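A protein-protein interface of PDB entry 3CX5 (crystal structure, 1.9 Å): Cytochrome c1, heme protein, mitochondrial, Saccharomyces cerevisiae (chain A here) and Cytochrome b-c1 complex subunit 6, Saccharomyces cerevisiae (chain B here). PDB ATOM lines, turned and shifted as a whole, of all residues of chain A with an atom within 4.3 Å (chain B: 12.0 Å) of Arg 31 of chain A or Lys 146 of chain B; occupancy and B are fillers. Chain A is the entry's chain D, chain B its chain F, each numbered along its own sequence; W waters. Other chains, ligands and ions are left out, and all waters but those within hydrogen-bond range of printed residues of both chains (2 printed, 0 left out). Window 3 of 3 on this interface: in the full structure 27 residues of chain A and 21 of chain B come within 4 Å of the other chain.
Water W2 bridges the chain-end carboxylate (O) of Lys 146 of chain B and the guanidinium group (NH1) of Arg 31 of chain A. Water W1 lies within hydrogen-bond range of OE1 of Gln 185 of chain A and OE1 of Gln 76 of chain B.
The guanidinium group of Arg 31 of chain A lies within salt-bridge range of the side-chain carboxylate of Asp 189 of chain A. The side-chain carboxylate (OD2) of Asp 177 of chain A is in salt-bridge range of the guanidinium group (NE) of Arg 31 of chain A (2.9 Å). NE2 of Gln 185 of chain A is in hydrogen-bond range of OD2 of Asp 189 of chain A, at 3.0 Å. The side-chain hydroxyl (OG1) of Thr 179 of chain A is in hydrogen-bond range of the side-chain carboxylate (OD1) of Asp 177 of chain A (3.1 Å). The guanidinium group of Arg 31 of chain A sits at hydrogen-bond distance from the side-chain hydroxyl of Thr 179 of chain A, at 3.3 Å.
Printed residues of chain B that touch a printed residue of chain A: Phe 142, Leu 145 and Lys 146. Among the printed residues, 6 pairs touch across the chains.
Among the printed residues, pairs that only touch across the chains: Thr 179 of chain A with Lys 146 of chain B (3.6 Å), Gln 185 of chain A with Leu 145 of chain B (3.6 Å) and Lys 188 of chain A with Phe 142 of chain B (3.5 Å).
Of the printed residues of chain B, Arg 31 of chain A touches Lys 146 (3.5 Å). Lys 146 of chain B touches just these residues of chain A: Arg 31, Thr 179, Gln 185 and Lys 188. No residue of chain B comes within 4 Å of Arg 30 of chain A. No residue of chain B comes within 4 Å of Gly 32 of chain A. Gln 34 of chain A touches none of the printed residues of chain B. Val 35 of chain A touches none of the printed residues of chain B. Of chain B, only Lys 146 comes within 4 Å of Thr 179 of chain A. Gln 185 of chain A touches just these residues of chain B: Leu 145 and Lys 146. No residue of chain B comes within 4 Å of Asp 189 of chain A. Of the printed residues of chain A, Leu 145 of chain B touches Gln 185. Of the printed residues of chain A, Phe 142 of chain B touches Lys 188. The nearest residue of chain B that does not touch Arg 31 of chain A is Leu 145 of chain B (7.0 Å). The nearest residue of chain A that does not touch Lys 146 of chain B is Asp 189 of chain A (4.2 Å).
The side-chain amide oxygen (OE1) of Gln 185 of chain A is in hydrogen-bond range of the backbone NH (N) of Lys 146 of chain B (2.7 Å). NH2 of Arg 31 of chain A lies within salt-bridge range of OXT of Lys 146 of chain B (3.7 Å). OXT of Lys 146 of chain B lies within salt-bridge range of NZ of Lys 188 of chain A, 3.0 Å away.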
ATOM      1  N   ALA A  27       1.534  13.216   6.553  1.00  0.00           N
ATOM      2  CA  ALA A  27       2.340  13.264   5.336  1.00  0.00           C
ATOM      3  C   ALA A  27       3.564  14.118   5.664  1.00  0.00           C
ATOM      4  O   ALA A  27       4.657  13.878   5.153  1.00  0.00           O
ATOM      5  CB  ALA A  27       1.550  13.881   4.175  1.00  0.00           C
ATOM      6  N   SER A  28       3.373  15.088   6.559  1.00  0.00           N
ATOM      7  CA  SER A  28       4.449  15.984   6.976  1.00  0.00           C
ATOM      8  C   SER A  28       5.437  15.266   7.910  1.00  0.00           C
ATOM      9  O   SER A  28       6.645  15.518   7.856  1.00  0.00           O
ATOM     10  CB  SER A  28       3.863  17.234   7.640  1.00  0.00           C
ATOM     11  OG  SER A  28       4.872  18.180   7.943  1.00  0.00           O
ATOM     12  N   ILE A  29       4.919  14.371   8.754  1.00  0.00           N
ATOM     13  CA  ILE A  29       5.758  13.586   9.669  1.00  0.00           C
ATOM     14  C   ILE A  29       6.698  12.725   8.823  1.00  0.00           C
ATOM     15  O   ILE A  29       7.900  12.631   9.097  1.00  0.00           O
ATOM     16  CB  ILE A  29       4.913  12.633  10.564  1.00  0.00           C
ATOM     17  CG1 ILE A  29       4.094  13.428  11.587  1.00  0.00           C
ATOM     18  CG2 ILE A  29       5.821  11.619  11.284  1.00  0.00           C
ATOM     19  CD1 ILE A  29       3.124  12.564  12.370  1.00  0.00           C
ATOM     20  N   ARG A  30       6.125  12.101   7.796  1.00  0.00           N
ATOM     21  CA  ARG A  30       6.857  11.238   6.870  1.00  0.00           C
ATOM     22  C   ARG A  30       7.992  11.965   6.160  1.00  0.00           C
ATOM     23  O   ARG A  30       9.114  11.465   6.115  1.00  0.00           O
ATOM     24  CB  ARG A  30       5.901  10.625   5.844  1.00  0.00           C
ATOM     25  CG  ARG A  30       6.575   9.699   4.844  1.00  0.00           C
ATOM     26  CD  ARG A  30       5.542   8.984   3.992  1.00  0.00           C
ATOM     27  NE  ARG A  30       6.164   8.177   2.950  1.00  0.00           N
ATOM     28  CZ  ARG A  30       6.366   6.865   3.019  1.00  0.00           C
ATOM     29  NH1 ARG A  30       6.948   6.237   2.001  1.00  0.00           N
ATOM     30  NH2 ARG A  30       5.977   6.173   4.087  1.00  0.00           N
ATOM     31  N   ARG A  31       7.709  13.143   5.606  1.00  0.00           N
ATOM     32  CA  ARG A  31       8.756  13.908   4.926  1.00  0.00           C
ATOM     33  C   ARG A  31       9.780  14.360   5.957  1.00  0.00           C
ATOM     34  O   ARG A  31      10.972  14.450   5.666  1.00  0.00           O
ATOM     35  CB  ARG A  31       8.188  15.155   4.246  1.00  0.00           C
ATOM     36  CG  ARG A  31       7.354  14.908   3.014  1.00  0.00           C
ATOM     37  CD  ARG A  31       6.885  16.238   2.436  1.00  0.00           C
ATOM     38  NE  ARG A  31       5.504  16.128   1.988  1.00  0.00           N
ATOM     39  CZ  ARG A  31       4.474  16.740   2.556  1.00  0.00           C
ATOM     40  NH1 ARG A  31       3.255  16.551   2.067  1.00  0.00           N
ATOM     41  NH2 ARG A  31       4.660  17.565   3.582  1.00  0.00           N
ATOM     42  N   GLY A  32       9.287  14.674   7.153  1.00  0.00           N
ATOM     43  CA  GLY A  32      10.150  15.132   8.228  1.00  0.00           C
ATOM     44  C   GLY A  32      11.188  14.104   8.609  1.00  0.00           C
ATOM     45  O   GLY A  32      12.317  14.466   8.939  1.00  0.00           O
ATOM     46  N   TYR A  33      10.804  12.828   8.579  1.00  0.00           N
ATOM     47  CA  TYR A  33      11.729  11.742   8.905  1.00  0.00           C
ATOM     48  C   TYR A  33      12.865  11.748   7.885  1.00  0.00           C
ATOM     49  O   TYR A  33      14.039  11.592   8.245  1.00  0.00           O
ATOM     50  CB  TYR A  33      11.037  10.368   8.895  1.00  0.00           C
ATOM     51  CG  TYR A  33      12.031   9.231   9.092  1.00  0.00           C
ATOM     52  CD1 TYR A  33      12.460   8.869  10.374  1.00  0.00           C
ATOM     53  CD2 TYR A  33      12.628   8.594   7.994  1.00  0.00           C
ATOM     54  CE1 TYR A  33      13.461   7.916  10.559  1.00  0.00           C
ATOM     55  CE2 TYR A  33      13.639   7.641   8.170  1.00  0.00           C
ATOM     56  CZ  TYR A  33      14.051   7.310   9.458  1.00  0.00           C
ATOM     57  OH  TYR A  33      15.073   6.404   9.649  1.00  0.00           O
ATOM     58  N   GLN A  34      12.509  11.918   6.613  1.00  0.00           N
ATOM     59  CA  GLN A  34      13.504  11.960   5.546  1.00  0.00           C
ATOM     60  C   GLN A  34      14.488  13.106   5.766  1.00  0.00           C
ATOM     61  O   GLN A  34      15.690  12.935   5.554  1.00  0.00           O
ATOM     62  CB  GLN A  34      12.837  12.088   4.177  1.00  0.00           C
ATOM     63  CG  GLN A  34      13.829  12.262   3.030  1.00  0.00           C
ATOM     64  CD  GLN A  34      13.180  12.158   1.657  1.00  0.00           C
ATOM     65  OE1 GLN A  34      11.958  12.237   1.527  1.00  0.00           O
ATOM     66  NE2 GLN A  34      14.003  11.965   0.628  1.00  0.00           N
ATOM     67  N   VAL A  35      13.996  14.268   6.193  1.00  0.00           N
ATOM     68  CA  VAL A  35      14.902  15.389   6.443  1.00  0.00           C
ATOM     69  C   VAL A  35      15.818  15.017   7.606  1.00  0.00           C
ATOM     70  O   VAL A  35      17.025  15.261   7.551  1.00  0.00           O
ATOM     71  CB  VAL A  35      14.164  16.699   6.766  1.00  0.00           C
ATOM     72  CG1 VAL A  35      15.177  17.805   7.057  1.00  0.00           C
ATOM     73  CG2 VAL A  35      13.264  17.114   5.599  1.00  0.00           C
ATOM     74  N   TYR A 175      12.099  15.000  -2.126  1.00  0.00           N
ATOM     75  CA  TYR A 175      10.931  14.353  -1.543  1.00  0.00           C
ATOM     76  C   TYR A 175      10.293  13.320  -2.462  1.00  0.00           C
ATOM     77  O   TYR A 175      10.034  13.581  -3.634  1.00  0.00           O
ATOM     78  CB  TYR A 175       9.885  15.392  -1.117  1.00  0.00           C
ATOM     79  CG  TYR A 175      10.201  16.143   0.165  1.00  0.00           C
ATOM     80  CD1 TYR A 175       9.859  17.487   0.304  1.00  0.00           C
ATOM     81  CD2 TYR A 175      10.794  15.500   1.255  1.00  0.00           C
ATOM     82  CE1 TYR A 175      10.090  18.174   1.493  1.00  0.00           C
ATOM     83  CE2 TYR A 175      11.031  16.182   2.455  1.00  0.00           C
ATOM     84  CZ  TYR A 175      10.675  17.514   2.565  1.00  0.00           C
ATOM     85  OH  TYR A 175      10.891  18.198   3.742  1.00  0.00           O
ATOM     86  N   ASP A 177       7.266  12.202  -2.567  1.00  0.00           N
ATOM     87  CA  ASP A 177       5.956  12.617  -3.073  1.00  0.00           C
ATOM     88  C   ASP A 177       5.952  13.790  -4.059  1.00  0.00           C
ATOM     89  O   ASP A 177       4.892  14.203  -4.534  1.00  0.00           O
ATOM     90  CB  ASP A 177       4.990  12.890  -1.908  1.00  0.00           C
ATOM     91  CG  ASP A 177       5.398  14.087  -1.051  1.00  0.00           C
ATOM     92  OD1 ASP A 177       6.525  14.614  -1.204  1.00  0.00           O
ATOM     93  OD2 ASP A 177       4.570  14.503  -0.212  1.00  0.00           O
ATOM     94  N   THR A 179       6.989  16.965  -3.398  1.00  0.00           N
ATOM     95  CA  THR A 179       6.871  18.271  -2.756  1.00  0.00           C
ATOM     96  C   THR A 179       8.177  19.051  -2.917  1.00  0.00           C
ATOM     97  O   THR A 179       9.259  18.487  -2.762  1.00  0.00           O
ATOM     98  CB  THR A 179       6.560  18.123  -1.245  1.00  0.00           C
ATOM     99  OG1 THR A 179       5.306  17.452  -1.069  1.00  0.00           O
ATOM    100  CG2 THR A 179       6.509  19.490  -0.567  1.00  0.00           C
ATOM    101  N   GLN A 185      10.008  24.571   3.708  1.00  0.00           N
ATOM    102  CA  GLN A 185       9.199  23.357   3.627  1.00  0.00           C
ATOM    103  C   GLN A 185       9.869  22.245   4.447  1.00  0.00           C
ATOM    104  O   GLN A 185       9.205  21.527   5.193  1.00  0.00           O
ATOM    105  CB  GLN A 185       9.042  22.902   2.174  1.00  0.00           C
ATOM    106  CG  GLN A 185       8.228  21.625   1.988  1.00  0.00           C
ATOM    107  CD  GLN A 185       6.752  21.798   2.304  1.00  0.00           C
ATOM    108  OE1 GLN A 185       6.074  22.646   1.725  1.00  0.00           O
ATOM    109  NE2 GLN A 185       6.240  20.970   3.210  1.00  0.00           N
ATOM    110  N   LYS A 188       9.573  23.003   8.143  1.00  0.00           N
ATOM    111  CA  LYS A 188       8.210  22.758   8.580  1.00  0.00           C
ATOM    112  C   LYS A 188       8.008  21.256   8.792  1.00  0.00           C
ATOM    113  O   LYS A 188       7.400  20.836   9.785  1.00  0.00           O
ATOM    114  CB  LYS A 188       7.224  23.286   7.534  1.00  0.00           C
ATOM    115  CG  LYS A 188       5.762  23.176   7.922  1.00  0.00           C
ATOM    116  CD  LYS A 188       5.058  22.068   7.162  1.00  0.00           C
ATOM    117  CE  LYS A 188       3.554  22.112   7.391  1.00  0.00           C
ATOM    118  NZ  LYS A 188       2.879  20.909   6.836  1.00  0.00           N
ATOM    119  N   ASP A 189       8.527  20.459   7.857  1.00  0.00           N
ATOM    120  CA  ASP A 189       8.412  19.007   7.928  1.00  0.00           C
ATOM    121  C   ASP A 189       9.213  18.350   9.063  1.00  0.00           C
ATOM    122  O   ASP A 189       8.664  17.490   9.757  1.00  0.00           O
ATOM    123  CB  ASP A 189       8.725  18.348   6.572  1.00  0.00           C
ATOM    124  CG  ASP A 189       7.704  18.713   5.481  1.00  0.00           C
ATOM    125  OD1 ASP A 189       6.507  18.889   5.792  1.00  0.00           O
ATOM    126  OD2 ASP A 189       8.103  18.830   4.301  1.00  0.00           O
ATOM    127  N   VAL B  73      11.367  25.939  -7.627  1.00  0.00           N
ATOM    128  CA  VAL B  73      10.622  26.827  -6.686  1.00  0.00           C
ATOM    129  C   VAL B  73      11.580  27.472  -5.687  1.00  0.00           C
ATOM    130  O   VAL B  73      12.456  26.806  -5.125  1.00  0.00           O
ATOM    131  CB  VAL B  73       9.524  26.045  -5.913  1.00  0.00           C
ATOM    132  CG1 VAL B  73       8.715  26.993  -5.030  1.00  0.00           C
ATOM    133  CG2 VAL B  73       8.609  25.312  -6.888  1.00  0.00           C
ATOM    134  N   THR B  74      11.431  28.780  -5.507  1.00  0.00           N
ATOM    135  CA  THR B  74      12.263  29.539  -4.578  1.00  0.00           C
ATOM    136  C   THR B  74      11.609  29.537  -3.189  1.00  0.00           C
ATOM    137  O   THR B  74      10.382  29.489  -3.078  1.00  0.00           O
ATOM    138  CB  THR B  74      12.468  30.987  -5.082  1.00  0.00           C
ATOM    139  OG1 THR B  74      13.290  31.708  -4.156  1.00  0.00           O
ATOM    140  CG2 THR B  74      11.126  31.704  -5.247  1.00  0.00           C
ATOM    141  N   ASP B  75      12.428  29.594  -2.141  1.00  0.00           N
ATOM    142  CA  ASP B  75      11.934  29.577  -0.763  1.00  0.00           C
ATOM    143  C   ASP B  75      10.816  30.580  -0.471  1.00  0.00           C
ATOM    144  O   ASP B  75      10.957  31.779  -0.720  1.00  0.00           O
ATOM    145  CB  ASP B  75      13.081  29.774   0.231  1.00  0.00           C
ATOM    146  CG  ASP B  75      12.642  29.546   1.666  1.00  0.00           C
ATOM    147  OD1 ASP B  75      12.217  28.412   1.981  1.00  0.00           O
ATOM    148  OD2 ASP B  75      12.699  30.501   2.469  1.00  0.00           O
ATOM    149  N   GLN B  76       9.726  30.074   0.102  1.00  0.00           N
ATOM    150  CA  GLN B  76       8.555  30.881   0.424  1.00  0.00           C
ATOM    151  C   GLN B  76       8.744  31.899   1.549  1.00  0.00           C
ATOM    152  O   GLN B  76       8.140  32.971   1.514  1.00  0.00           O
ATOM    153  CB  GLN B  76       7.349  29.986   0.715  1.00  0.00           C
ATOM    154  CG  GLN B  76       6.972  29.043  -0.428  1.00  0.00           C
ATOM    155  CD  GLN B  76       7.676  27.692  -0.365  1.00  0.00           C
ATOM    156  OE1 GLN B  76       7.195  26.706  -0.924  1.00  0.00           O
ATOM    157  NE2 GLN B  76       8.802  27.635   0.330  1.00  0.00           N
ATOM    158  N   LEU B  77       9.555  31.574   2.554  1.00  0.00           N
ATOM    159  CA  LEU B  77       9.780  32.527   3.637  1.00  0.00           C
ATOM    160  C   LEU B  77      10.674  33.658   3.132  1.00  0.00           C
ATOM    161  O   LEU B  77      10.401  34.826   3.399  1.00  0.00           O
ATOM    162  CB  LEU B  77      10.387  31.851   4.869  1.00  0.00           C
ATOM    163  CG  LEU B  77      10.590  32.737   6.108  1.00  0.00           C
ATOM    164  CD1 LEU B  77       9.309  33.482   6.472  1.00  0.00           C
ATOM    165  CD2 LEU B  77      11.061  31.881   7.275  1.00  0.00           C
ATOM    166  N   LEU B  80       8.523  35.925   1.001  1.00  0.00           N
ATOM    167  CA  LEU B  80       7.655  36.749   1.835  1.00  0.00           C
ATOM    168  C   LEU B  80       8.441  37.834   2.561  1.00  0.00           C
ATOM    169  O   LEU B  80       7.979  38.969   2.662  1.00  0.00           O
ATOM    170  CB  LEU B  80       6.894  35.888   2.845  1.00  0.00           C
ATOM    171  CG  LEU B  80       5.614  35.205   2.358  1.00  0.00           C
ATOM    172  CD1 LEU B  80       5.102  34.234   3.412  1.00  0.00           C
ATOM    173  CD2 LEU B  80       4.556  36.256   2.054  1.00  0.00           C
ATOM    174  N   ARG B 140       1.151  34.187   7.396  1.00  0.00           N
ATOM    175  CA  ARG B 140       0.965  33.935   5.968  1.00  0.00           C
ATOM    176  C   ARG B 140       1.767  32.779   5.381  1.00  0.00           C
ATOM    177  O   ARG B 140       1.344  32.160   4.409  1.00  0.00           O
ATOM    178  CB  ARG B 140       1.288  35.204   5.171  1.00  0.00           C
ATOM    179  CG  ARG B 140       0.111  36.140   4.964  1.00  0.00           C
ATOM    180  CD  ARG B 140       0.529  37.369   4.165  1.00  0.00           C
ATOM    181  NE  ARG B 140       1.126  38.382   5.028  1.00  0.00           N
ATOM    182  CZ  ARG B 140       0.459  39.419   5.531  1.00  0.00           C
ATOM    183  NH1 ARG B 140       1.077  40.283   6.322  1.00  0.00           N
ATOM    184  NH2 ARG B 140      -0.816  39.614   5.213  1.00  0.00           N
ATOM    185  N   LEU B 141       2.912  32.472   5.979  1.00  0.00           N
ATOM    186  CA  LEU B 141       3.778  31.417   5.459  1.00  0.00           C
ATOM    187  C   LEU B 141       3.190  30.037   5.180  1.00  0.00           C
ATOM    188  O   LEU B 141       3.274  29.555   4.049  1.00  0.00           O
ATOM    189  CB  LEU B 141       5.038  31.273   6.321  1.00  0.00           C
ATOM    190  CG  LEU B 141       6.028  30.195   5.856  1.00  0.00           C
ATOM    191  CD1 LEU B 141       6.534  30.495   4.436  1.00  0.00           C
ATOM    192  CD2 LEU B 141       7.187  30.118   6.821  1.00  0.00           C
ATOM    193  N   PHE B 142       2.588  29.403   6.184  1.00  0.00           N
ATOM    194  CA  PHE B 142       2.060  28.049   6.000  1.00  0.00           C
ATOM    195  C   PHE B 142       1.028  27.829   4.906  1.00  0.00           C
ATOM    196  O   PHE B 142       0.889  26.716   4.397  1.00  0.00           O
ATOM    197  CB  PHE B 142       1.624  27.435   7.337  1.00  0.00           C
ATOM    198  CG  PHE B 142       2.779  26.967   8.186  1.00  0.00           C
ATOM    199  CD1 PHE B 142       4.025  27.594   8.102  1.00  0.00           C
ATOM    200  CD2 PHE B 142       2.633  25.890   9.057  1.00  0.00           C
ATOM    201  CE1 PHE B 142       5.102  27.157   8.868  1.00  0.00           C
ATOM    202  CE2 PHE B 142       3.703  25.445   9.828  1.00  0.00           C
ATOM    203  CZ  PHE B 142       4.942  26.078   9.734  1.00  0.00           C
ATOM    204  N   ASP B 143       0.350  28.896   4.500  1.00  0.00           N
ATOM    205  CA  ASP B 143      -0.638  28.805   3.428  1.00  0.00           C
ATOM    206  C   ASP B 143       0.083  28.553   2.095  1.00  0.00           C
ATOM    207  O   ASP B 143      -0.517  28.064   1.136  1.00  0.00           O
ATOM    208  CB  ASP B 143      -1.454  30.097   3.350  1.00  0.00           C
ATOM    209  CG  ASP B 143      -2.156  30.422   4.659  1.00  0.00           C
ATOM    210  OD1 ASP B 143      -3.405  30.407   4.682  1.00  0.00           O
ATOM    211  OD2 ASP B 143      -1.458  30.686   5.670  1.00  0.00           O
ATOM    212  N   LYS B 144       1.381  28.860   2.071  1.00  0.00           N
ATOM    213  CA  LYS B 144       2.228  28.679   0.889  1.00  0.00           C
ATOM    214  C   LYS B 144       3.017  27.361   0.920  1.00  0.00           C
ATOM    215  O   LYS B 144       3.745  27.043  -0.026  1.00  0.00           O
ATOM    216  CB  LYS B 144       3.225  29.843   0.774  1.00  0.00           C
ATOM    217  CG  LYS B 144       2.606  31.226   0.611  1.00  0.00           C
ATOM    218  CD  LYS B 144       2.048  31.435  -0.792  1.00  0.00           C
ATOM    219  CE  LYS B 144       1.448  32.828  -0.953  1.00  0.00           C
ATOM    220  NZ  LYS B 144       2.451  33.904  -0.689  1.00  0.00           N
ATOM    221  N   LEU B 145       2.904  26.616   2.016  1.00  0.00           N
ATOM    222  CA  LEU B 145       3.627  25.355   2.154  1.00  0.00           C
ATOM    223  C   LEU B 145       2.745  24.118   2.053  1.00  0.00           C
ATOM    224  O   LEU B 145       1.520  24.197   2.127  1.00  0.00           O
ATOM    225  CB  LEU B 145       4.407  25.329   3.471  1.00  0.00           C
ATOM    226  CG  LEU B 145       5.505  26.383   3.635  1.00  0.00           C
ATOM    227  CD1 LEU B 145       6.183  26.219   4.989  1.00  0.00           C
ATOM    228  CD2 LEU B 145       6.527  26.250   2.517  1.00  0.00           C
ATOM    229  N   LYS B 146       3.390  22.972   1.879  1.00  0.00           N
ATOM    230  CA  LYS B 146       2.699  21.694   1.763  1.00  0.00           C
ATOM    231  C   LYS B 146       2.514  21.077   3.154  1.00  0.00           C
ATOM    232  O   LYS B 146       1.402  20.585   3.438  1.00  0.00           O
ATOM    233  CB  LYS B 146       3.516  20.756   0.869  1.00  0.00           C
ATOM    234  CG  LYS B 146       2.784  19.524   0.377  1.00  0.00           C
ATOM    235  CD  LYS B 146       1.763  19.873  -0.694  1.00  0.00           C
ATOM    236  CE  LYS B 146       1.172  18.612  -1.317  1.00  0.00           C
ATOM    237  NZ  LYS B 146       0.484  17.756  -0.310  1.00  0.00           N
ATOM    238  OXT LYS B 146       3.482  21.096   3.947  1.00  0.00           O
HETATM  239  O   HOH W   1       7.411  23.376  -0.681  1.00  0.00           O
HETATM  240  O   HOH W   2       1.562  18.021   4.134  1.00  0.00           O
